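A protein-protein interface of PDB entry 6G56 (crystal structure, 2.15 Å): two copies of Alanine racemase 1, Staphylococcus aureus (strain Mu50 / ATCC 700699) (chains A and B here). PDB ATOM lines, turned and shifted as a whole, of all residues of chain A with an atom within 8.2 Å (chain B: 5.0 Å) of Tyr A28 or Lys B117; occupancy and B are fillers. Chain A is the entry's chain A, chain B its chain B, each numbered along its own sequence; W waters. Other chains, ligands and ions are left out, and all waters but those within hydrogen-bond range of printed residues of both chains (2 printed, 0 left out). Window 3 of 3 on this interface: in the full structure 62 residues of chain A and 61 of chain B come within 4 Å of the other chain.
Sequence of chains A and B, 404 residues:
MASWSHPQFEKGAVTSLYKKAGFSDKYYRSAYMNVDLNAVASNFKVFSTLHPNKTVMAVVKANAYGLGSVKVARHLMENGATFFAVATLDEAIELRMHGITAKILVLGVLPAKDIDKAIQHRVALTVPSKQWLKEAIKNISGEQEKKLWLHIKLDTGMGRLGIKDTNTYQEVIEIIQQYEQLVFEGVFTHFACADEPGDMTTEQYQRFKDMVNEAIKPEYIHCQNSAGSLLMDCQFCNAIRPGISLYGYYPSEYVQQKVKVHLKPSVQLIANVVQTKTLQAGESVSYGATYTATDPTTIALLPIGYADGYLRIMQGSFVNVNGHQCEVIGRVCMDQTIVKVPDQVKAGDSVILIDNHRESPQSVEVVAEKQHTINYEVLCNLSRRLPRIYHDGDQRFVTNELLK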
ATOM      1  N   ASP A  25       2.360  -2.098   6.975  1.00  0.00           N
ATOM      2  CA  ASP A  25       1.272  -1.376   6.309  1.00  0.00           C
ATOM      3  C   ASP A  25       1.620   0.110   6.125  1.00  0.00           C
ATOM      4  O   ASP A  25       2.394   0.698   6.872  1.00  0.00           O
ATOM      5  CB  ASP A  25      -0.036  -1.442   7.124  1.00  0.00           C
ATOM      6  CG  ASP A  25      -0.590  -2.842   7.289  1.00  0.00           C
ATOM      7  OD1 ASP A  25      -0.508  -3.639   6.343  1.00  0.00           O
ATOM      8  OD2 ASP A  25      -1.156  -3.130   8.372  1.00  0.00           O
ATOM      9  N   LYS A  26       1.022   0.713   5.120  1.00  0.00           N
ATOM     10  CA  LYS A  26       1.031   2.159   4.990  1.00  0.00           C
ATOM     11  C   LYS A  26       0.006   2.765   5.968  1.00  0.00           C
ATOM     12  O   LYS A  26      -0.869   2.070   6.525  1.00  0.00           O
ATOM     13  CB  LYS A  26       0.727   2.551   3.534  1.00  0.00           C
ATOM     14  CG  LYS A  26       1.787   2.085   2.536  1.00  0.00           C
ATOM     15  CD  LYS A  26       3.176   2.641   2.881  1.00  0.00           C
ATOM     16  CE  LYS A  26       4.078   2.877   1.672  1.00  0.00           C
ATOM     17  NZ  LYS A  26       4.517   1.612   1.023  1.00  0.00           N
ATOM     18  N   TYR A  27       0.149   4.059   6.225  1.00  0.00           N
ATOM     19  CA  TYR A  27      -0.912   4.814   6.912  1.00  0.00           C
ATOM     20  C   TYR A  27      -0.938   6.264   6.409  1.00  0.00           C
ATOM     21  O   TYR A  27       0.071   6.792   5.952  1.00  0.00           O
ATOM     22  CB  TYR A  27      -0.805   4.685   8.436  1.00  0.00           C
ATOM     23  CG  TYR A  27       0.353   5.436   9.018  1.00  0.00           C
ATOM     24  CD1 TYR A  27       1.636   4.925   8.949  1.00  0.00           C
ATOM     25  CD2 TYR A  27       0.164   6.655   9.624  1.00  0.00           C
ATOM     26  CE1 TYR A  27       2.710   5.611   9.473  1.00  0.00           C
ATOM     27  CE2 TYR A  27       1.224   7.372  10.146  1.00  0.00           C
ATOM     28  CZ  TYR A  27       2.493   6.845  10.079  1.00  0.00           C
ATOM     29  OH  TYR A  27       3.527   7.572  10.588  1.00  0.00           O
ATOM     30  N   TYR A  28      -2.103   6.884   6.473  1.00  0.00           N
ATOM     31  CA  TYR A  28      -2.404   8.094   5.684  1.00  0.00           C
ATOM     32  C   TYR A  28      -3.045   9.225   6.476  1.00  0.00           C
ATOM     33  O   TYR A  28      -3.834  10.012   5.934  1.00  0.00           O
ATOM     34  CB  TYR A  28      -3.258   7.712   4.468  1.00  0.00           C
ATOM     35  CG  TYR A  28      -2.575   6.728   3.545  1.00  0.00           C
ATOM     36  CD1 TYR A  28      -1.444   7.098   2.834  1.00  0.00           C
ATOM     37  CD2 TYR A  28      -3.040   5.407   3.397  1.00  0.00           C
ATOM     38  CE1 TYR A  28      -0.796   6.211   1.982  1.00  0.00           C
ATOM     39  CE2 TYR A  28      -2.398   4.506   2.541  1.00  0.00           C
ATOM     40  CZ  TYR A  28      -1.270   4.914   1.829  1.00  0.00           C
ATOM     41  OH  TYR A  28      -0.596   4.067   0.969  1.00  0.00           O
ATOM     42  N   ARG A  29      -2.669   9.307   7.749  1.00  0.00           N
ATOM     43  CA  ARG A  29      -3.038  10.400   8.655  1.00  0.00           C
ATOM     44  C   ARG A  29      -1.967  10.424   9.757  1.00  0.00           C
ATOM     45  O   ARG A  29      -1.564   9.367  10.252  1.00  0.00           O
ATOM     46  CB  ARG A  29      -4.434  10.178   9.292  1.00  0.00           C
ATOM     47  CG  ARG A  29      -4.802  11.221  10.349  1.00  0.00           C
ATOM     48  CD  ARG A  29      -6.095  10.918  11.070  1.00  0.00           C
ATOM     49  NE  ARG A  29      -5.982   9.707  11.870  1.00  0.00           N
ATOM     50  CZ  ARG A  29      -6.734   9.368  12.917  1.00  0.00           C
ATOM     51  NH1 ARG A  29      -7.696  10.136  13.374  1.00  0.00           N
ATOM     52  NH2 ARG A  29      -6.495   8.222  13.542  1.00  0.00           N
ATOM     53  N   SER A  30      -1.563  11.623  10.163  1.00  0.00           N
ATOM     54  CA  SER A  30      -0.466  11.818  11.089  1.00  0.00           C
ATOM     55  C   SER A  30      -0.920  11.752  12.535  1.00  0.00           C
ATOM     56  O   SER A  30      -0.823  12.719  13.266  1.00  0.00           O
ATOM     57  CB  SER A  30       0.240  13.152  10.769  1.00  0.00           C
ATOM     58  OG  SER A  30       0.653  13.185   9.397  1.00  0.00           O
ATOM     59  N   ALA A  31      -1.419  10.584  12.921  1.00  0.00           N
ATOM     60  CA  ALA A  31      -1.744  10.209  14.298  1.00  0.00           C
ATOM     61  C   ALA A  31      -1.514   8.704  14.425  1.00  0.00           C
ATOM     62  O   ALA A  31      -1.940   7.933  13.554  1.00  0.00           O
ATOM     63  CB  ALA A  31      -3.185  10.528  14.630  1.00  0.00           C
ATOM     64  N   PRO A 303      -5.145  15.989  14.100  1.00  0.00           N
ATOM     65  CA  PRO A 303      -6.032  15.055  13.421  1.00  0.00           C
ATOM     66  C   PRO A 303      -6.231  13.808  14.277  1.00  0.00           C
ATOM     67  O   PRO A 303      -5.897  12.682  13.863  1.00  0.00           O
ATOM     68  CB  PRO A 303      -5.269  14.765  12.133  1.00  0.00           C
ATOM     69  CG  PRO A 303      -3.846  14.771  12.566  1.00  0.00           C
ATOM     70  CD  PRO A 303      -3.749  15.822  13.643  1.00  0.00           C
ATOM     71  N   ARG A 385      -8.583   2.709  14.627  1.00  0.00           N
ATOM     72  CA  ARG A 385      -8.183   3.709  13.660  1.00  0.00           C
ATOM     73  C   ARG A 385      -6.730   4.167  13.808  1.00  0.00           C
ATOM     74  O   ARG A 385      -6.121   4.610  12.835  1.00  0.00           O
ATOM     75  CB  ARG A 385      -9.158   4.875  13.658  1.00  0.00           C
ATOM     76  CG  ARG A 385      -8.979   5.750  12.438  1.00  0.00           C
ATOM     77  CD  ARG A 385     -10.138   6.674  12.197  1.00  0.00           C
ATOM     78  NE  ARG A 385     -10.214   7.720  13.203  1.00  0.00           N
ATOM     79  CZ  ARG A 385     -11.132   8.677  13.208  1.00  0.00           C
ATOM     80  NH1 ARG A 385     -12.072   8.709  12.264  1.00  0.00           N
ATOM     81  NH2 ARG A 385     -11.135   9.580  14.170  1.00  0.00           N
ATOM     82  N   PRO A 387      -2.973   3.572  13.776  1.00  0.00           N
ATOM     83  CA  PRO A 387      -1.910   2.643  13.450  1.00  0.00           C
ATOM     84  C   PRO A 387      -1.020   2.402  14.678  1.00  0.00           C
ATOM     85  O   PRO A 387      -0.769   3.345  15.444  1.00  0.00           O
ATOM     86  CB  PRO A 387      -1.112   3.368  12.344  1.00  0.00           C
ATOM     87  CG  PRO A 387      -2.011   4.416  11.836  1.00  0.00           C
ATOM     88  CD  PRO A 387      -2.866   4.819  12.986  1.00  0.00           C
ATOM     89  N   VAL A 398       4.634  -1.215  10.889  1.00  0.00           N
ATOM     90  CA  VAL A 398       3.363  -0.563  11.110  1.00  0.00           C
ATOM     91  C   VAL A 398       2.239  -1.558  10.888  1.00  0.00           C
ATOM     92  O   VAL A 398       2.277  -2.327   9.929  1.00  0.00           O
ATOM     93  CB  VAL A 398       3.168   0.544  10.057  1.00  0.00           C
ATOM     94  CG1 VAL A 398       1.801   1.224  10.257  1.00  0.00           C
ATOM     95  CG2 VAL A 398       4.325   1.533  10.096  1.00  0.00           C
ATOM     96  N   ASN A 400      -1.868  -1.227  10.435  1.00  0.00           N
ATOM     97  CA  ASN A 400      -2.954  -0.273  10.203  1.00  0.00           C
ATOM     98  C   ASN A 400      -4.165  -1.128   9.912  1.00  0.00           C
ATOM     99  O   ASN A 400      -4.282  -1.651   8.816  1.00  0.00           O
ATOM    100  CB  ASN A 400      -2.584   0.645   9.040  1.00  0.00           C
ATOM    101  CG  ASN A 400      -3.665   1.692   8.712  1.00  0.00           C
ATOM    102  OD1 ASN A 400      -4.700   1.780   9.380  1.00  0.00           O
ATOM    103  ND2 ASN A 400      -3.395   2.505   7.675  1.00  0.00           N
ATOM    104  N   LEU A 403      -6.522  -1.007   6.682  1.00  0.00           N
ATOM    105  CA  LEU A 403      -6.043  -1.513   5.388  1.00  0.00           C
ATOM    106  C   LEU A 403      -5.701  -3.000   5.381  1.00  0.00           C
ATOM    107  O   LEU A 403      -5.039  -3.458   4.448  1.00  0.00           O
ATOM    108  CB  LEU A 403      -4.838  -0.686   4.923  1.00  0.00           C
ATOM    109  CG  LEU A 403      -5.049   0.822   4.917  1.00  0.00           C
ATOM    110  CD1 LEU A 403      -3.749   1.496   4.477  1.00  0.00           C
ATOM    111  CD2 LEU A 403      -6.210   1.189   3.997  1.00  0.00           C
ATOM    112  N   LEU B  89      -7.993   9.495   4.721  1.00  0.00           N
ATOM    113  CA  LEU B  89      -7.742   8.720   3.518  1.00  0.00           C
ATOM    114  C   LEU B  89      -7.718   7.209   3.784  1.00  0.00           C
ATOM    115  O   LEU B  89      -8.145   6.443   2.908  1.00  0.00           O
ATOM    116  CB  LEU B  89      -6.424   9.134   2.844  1.00  0.00           C
ATOM    117  CG  LEU B  89      -6.111   8.411   1.532  1.00  0.00           C
ATOM    118  CD1 LEU B  89      -7.224   8.621   0.515  1.00  0.00           C
ATOM    119  CD2 LEU B  89      -4.773   8.875   0.976  1.00  0.00           C
ATOM    120  N   ASP B  90      -7.255   6.779   4.964  1.00  0.00           N
ATOM    121  CA  ASP B  90      -7.267   5.343   5.292  1.00  0.00           C
ATOM    122  C   ASP B  90      -8.691   4.820   5.238  1.00  0.00           C
ATOM    123  O   ASP B  90      -8.936   3.706   4.714  1.00  0.00           O
ATOM    124  CB  ASP B  90      -6.689   5.022   6.692  1.00  0.00           C
ATOM    125  CG  ASP B  90      -5.340   5.644   6.925  1.00  0.00           C
ATOM    126  OD1 ASP B  90      -5.336   6.805   7.393  1.00  0.00           O
ATOM    127  OD2 ASP B  90      -4.293   4.983   6.685  1.00  0.00           O
ATOM    128  N   ILE B  93      -9.674   4.508   1.534  1.00  0.00           N
ATOM    129  CA  ILE B  93      -9.024   3.385   0.882  1.00  0.00           C
ATOM    130  C   ILE B  93      -9.679   2.087   1.338  1.00  0.00           C
ATOM    131  O   ILE B  93      -9.922   1.207   0.521  1.00  0.00           O
ATOM    132  CB  ILE B  93      -7.486   3.414   1.055  1.00  0.00           C
ATOM    133  CG1 ILE B  93      -6.921   4.616   0.271  1.00  0.00           C
ATOM    134  CG2 ILE B  93      -6.850   2.120   0.534  1.00  0.00           C
ATOM    135  CD1 ILE B  93      -5.450   4.859   0.508  1.00  0.00           C
ATOM    136  N   LEU B 110      -5.351  15.966   4.599  1.00  0.00           N
ATOM    137  CA  LEU B 110      -4.470  14.902   4.180  1.00  0.00           C
ATOM    138  C   LEU B 110      -3.017  15.361   4.304  1.00  0.00           C
ATOM    139  O   LEU B 110      -2.686  16.471   3.894  1.00  0.00           O
ATOM    140  CB  LEU B 110      -4.772  14.508   2.737  1.00  0.00           C
ATOM    141  CG  LEU B 110      -3.950  13.299   2.238  1.00  0.00           C
ATOM    142  CD1 LEU B 110      -4.532  12.009   2.768  1.00  0.00           C
ATOM    143  CD2 LEU B 110      -3.858  13.248   0.721  1.00  0.00           C
ATOM    144  N   PRO B 111      -2.126  14.503   4.868  1.00  0.00           N
ATOM    145  CA  PRO B 111      -0.703  14.848   4.789  1.00  0.00           C
ATOM    146  C   PRO B 111      -0.324  15.025   3.320  1.00  0.00           C
ATOM    147  O   PRO B 111      -0.646  14.167   2.483  1.00  0.00           O
ATOM    148  CB  PRO B 111       0.003  13.615   5.373  1.00  0.00           C
ATOM    149  CG  PRO B 111      -1.020  12.970   6.235  1.00  0.00           C
ATOM    150  CD  PRO B 111      -2.341  13.216   5.539  1.00  0.00           C
ATOM    151  N   ASP B 114       0.987  12.340   0.874  1.00  0.00           N
ATOM    152  CA  ASP B 114       0.101  11.255   0.456  1.00  0.00           C
ATOM    153  C   ASP B 114      -0.798  11.641  -0.702  1.00  0.00           C
ATOM    154  O   ASP B 114      -1.733  10.896  -1.020  1.00  0.00           O
ATOM    155  CB  ASP B 114      -0.748  10.798   1.644  1.00  0.00           C
ATOM    156  CG  ASP B 114       0.090  10.334   2.825  1.00  0.00           C
ATOM    157  OD1 ASP B 114       1.147   9.719   2.577  1.00  0.00           O
ATOM    158  OD2 ASP B 114      -0.342  10.573   3.983  1.00  0.00           O
ATOM    159  N   ILE B 115      -0.527  12.779  -1.343  1.00  0.00           N
ATOM    160  CA  ILE B 115      -1.431  13.290  -2.381  1.00  0.00           C
ATOM    161  C   ILE B 115      -1.612  12.279  -3.529  1.00  0.00           C
ATOM    162  O   ILE B 115      -2.729  12.050  -3.965  1.00  0.00           O
ATOM    163  CB  ILE B 115      -0.959  14.704  -2.893  1.00  0.00           C
ATOM    164  CG1 ILE B 115      -2.041  15.386  -3.706  1.00  0.00           C
ATOM    165  CG2 ILE B 115       0.340  14.635  -3.704  1.00  0.00           C
ATOM    166  CD1 ILE B 115      -3.239  15.755  -2.871  1.00  0.00           C
ATOM    167  N   ASP B 116      -0.535  11.631  -3.962  1.00  0.00           N
ATOM    168  CA  ASP B 116      -0.620  10.662  -5.064  1.00  0.00           C
ATOM    169  C   ASP B 116      -1.552   9.489  -4.748  1.00  0.00           C
ATOM    170  O   ASP B 116      -2.194   8.947  -5.647  1.00  0.00           O
ATOM    171  CB  ASP B 116       0.769  10.134  -5.480  1.00  0.00           C
ATOM    172  CG  ASP B 116       1.604  11.174  -6.247  1.00  0.00           C
ATOM    173  OD1 ASP B 116       1.051  12.148  -6.822  1.00  0.00           O
ATOM    174  OD2 ASP B 116       2.847  11.004  -6.277  1.00  0.00           O
ATOM    175  N   LYS B 117      -1.639   9.097  -3.480  1.00  0.00           N
ATOM    176  CA  LYS B 117      -2.531   7.983  -3.103  1.00  0.00           C
ATOM    177  C   LYS B 117      -3.995   8.362  -3.176  1.00  0.00           C
ATOM    178  O   LYS B 117      -4.829   7.535  -3.559  1.00  0.00           O
ATOM    179  CB  LYS B 117      -2.213   7.430  -1.715  1.00  0.00           C
ATOM    180  CG  LYS B 117      -1.026   6.498  -1.733  1.00  0.00           C
ATOM    181  CD  LYS B 117      -1.375   5.106  -2.256  1.00  0.00           C
ATOM    182  CE  LYS B 117      -0.143   4.406  -2.791  1.00  0.00           C
ATOM    183  NZ  LYS B 117      -0.515   3.167  -3.524  1.00  0.00           N
ATOM    184  N   ALA B 118      -4.317   9.587  -2.772  1.00  0.00           N
ATOM    185  CA  ALA B 118      -5.661  10.110  -2.981  1.00  0.00           C
ATOM    186  C   ALA B 118      -6.017  10.099  -4.472  1.00  0.00           C
ATOM    187  O   ALA B 118      -7.116   9.660  -4.835  1.00  0.00           O
ATOM    188  CB  ALA B 118      -5.803  11.506  -2.404  1.00  0.00           C
ATOM    189  N   ILE B 119      -5.075  10.537  -5.316  1.00  0.00           N
ATOM    190  CA  ILE B 119      -5.331  10.627  -6.752  1.00  0.00           C
ATOM    191  C   ILE B 119      -5.539   9.236  -7.338  1.00  0.00           C
ATOM    192  O   ILE B 119      -6.524   8.991  -8.030  1.00  0.00           O
ATOM    193  CB  ILE B 119      -4.196  11.357  -7.530  1.00  0.00           C
ATOM    194  CG1 ILE B 119      -4.105  12.830  -7.116  1.00  0.00           C
ATOM    195  CG2 ILE B 119      -4.443  11.275  -9.046  1.00  0.00           C
ATOM    196  CD1 ILE B 119      -2.786  13.499  -7.512  1.00  0.00           C
ATOM    197  N   GLN B 120      -4.622   8.330  -7.022  1.00  0.00           N
ATOM    198  CA  GLN B 120      -4.694   6.935  -7.460  1.00  0.00           C
ATOM    199  C   GLN B 120      -6.066   6.308  -7.222  1.00  0.00           C
ATOM    200  O   GLN B 120      -6.611   5.659  -8.103  1.00  0.00           O
ATOM    201  CB  GLN B 120      -3.615   6.098  -6.738  1.00  0.00           C
ATOM    202  CG  GLN B 120      -3.563   4.631  -7.164  1.00  0.00           C
ATOM    203  CD  GLN B 120      -2.642   3.789  -6.313  1.00  0.00           C
ATOM    204  OE1 GLN B 120      -1.789   4.315  -5.617  1.00  0.00           O
ATOM    205  NE2 GLN B 120      -2.830   2.479  -6.335  1.00  0.00           N
ATOM    206  N   HIS B 121      -6.601   6.507  -6.019  1.00  0.00           N
ATOM    207  CA  HIS B 121      -7.850   5.865  -5.580  1.00  0.00           C
ATOM    208  C   HIS B 121      -9.083   6.729  -5.782  1.00  0.00           C
ATOM    209  O   HIS B 121     -10.143   6.412  -5.226  1.00  0.00           O
ATOM    210  CB  HIS B 121      -7.727   5.448  -4.099  1.00  0.00           C
ATOM    211  CG  HIS B 121      -6.735   4.361  -3.886  1.00  0.00           C
ATOM    212  ND1 HIS B 121      -6.963   3.069  -4.319  1.00  0.00           N
ATOM    213  CD2 HIS B 121      -5.495   4.370  -3.346  1.00  0.00           C
ATOM    214  CE1 HIS B 121      -5.906   2.324  -4.036  1.00  0.00           C
ATOM    215  NE2 HIS B 121      -5.008   3.085  -3.438  1.00  0.00           N
HETATM  216  O   HOH W   1       0.904   9.731   6.203  1.00  0.00           O
HETATM  217  O   HOH W   2      -6.102  11.214   5.873  1.00  0.00           O
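The side-chain amide nitrogen (ND2) of Asn A400 lies within hydrogen-bond range of the side-chain carboxylate (OD2) of Asp B90. The backbone NH of Tyr A28 sits at hydrogen-bond distance from the side-chain carboxylate of Asp B90 (2.9 Å).
NH1 of Arg A29 is in hydrogen-bond range of O of Pro A303 (3.2 Å). The backbone NH of Asn A400 is in hydrogen-bond range of the side-chain carboxylate of Asp A25 (2.9 Å). The side-chain amide oxygen (OE1) of Gln B120 sits at hydrogen-bond distance from the side-chain amino group (NZ) of Lys B117 (2.7 Å). O of Lys A26 sits at hydrogen-bond distance from ND2 of Asn A400 (2.8 Å).
OD2 of Asp B90 touches CA of Tyr A27, 3.4 Å away. CB of Tyr A28 touches CB of Leu B89 (3.8 Å). CE2 of Tyr A28 touches CD1 of Ile B93, at 3.7 Å. Tyr A28 touches Leu B110. Tyr A28 touches Asp B114. OH of Tyr A28 touches CD of Lys B117, at 3.5 Å. Asp B90 touches Arg A29. CG of Pro B111 touches OG of Ser A30, at 3.6 Å. Leu A403 touches Asp B90. Ile B93 touches Leu A403 (CG2 to CD2, 3.6 Å).
Tyr A28 touches just these residues of chain B: Leu B89 (3.8 Å), Asp B90 (2.9 Å), Ile B93 (3.7 Å), Leu B110 (3.8 Å), Pro B111 (3.6 Å), Asp B114 (3.6 Å) and Lys B117 (3.5 Å). Of chain A, only Tyr A28 (3.5 Å) comes within 4 Å of Lys B117. No residue of chain A comes within 4 Å of Ala B118. Of the printed residues of chain B, Arg A29 touches Asp B90 (3.7 Å). Of the printed residues of chain A, Asp B90 touches Tyr A27, Tyr A28, Arg A29, Asn A400 and Leu A403. Of the printed residues of chain A, Pro B111 touches Tyr A28 (3.6 Å) and Ser A30 (3.6 Å). Printed residues of chain B within 4 Å of Leu A403: Asp B90 (3.8 Å) and Ile B93 (3.6 Å). The nearest residue of chain A that does not touch Lys B117 is Lys A26 (6.1 Å).
Of the 13 printed residues of chain A, 6 touch a printed residue of chain B. Hydrophobic or aromatic side chains of chain A within 4 Å of the printed part of chain B: Tyr A27, Tyr A28 and Leu A403. Of the 13 printed residues of chain B, 7 touch a printed residue of chain A. Hydrophobic or aromatic side chains of chain B that line the printed part of chain A: Leu B89, Ile B93, Leu B110 and Pro B111. Along chain B the printed residues that touch a printed residue of chain A span positions 89 to 117. Among the printed residues, 13 pairs touch across the chains. Among the printed residues, no Asp or Glu carboxylate lies within 4 Å of a Lys or Arg side-chain nitrogen of the other chain.
No position is printed for both chains. Of the 13 pairs that touch across the chains among the printed residues, none has its exchanged pair printed and touching as well.
Water W2 lies within hydrogen-bond range of the backbone carbonyl oxygen (O) of Tyr A28 (2.6 Å) and the backbone NH (N) of Leu B89 (2.8 Å). Water W1 bridges OD2 of Asp B114 (2.7 Å) and O of Tyr A27 (3.1 Å).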
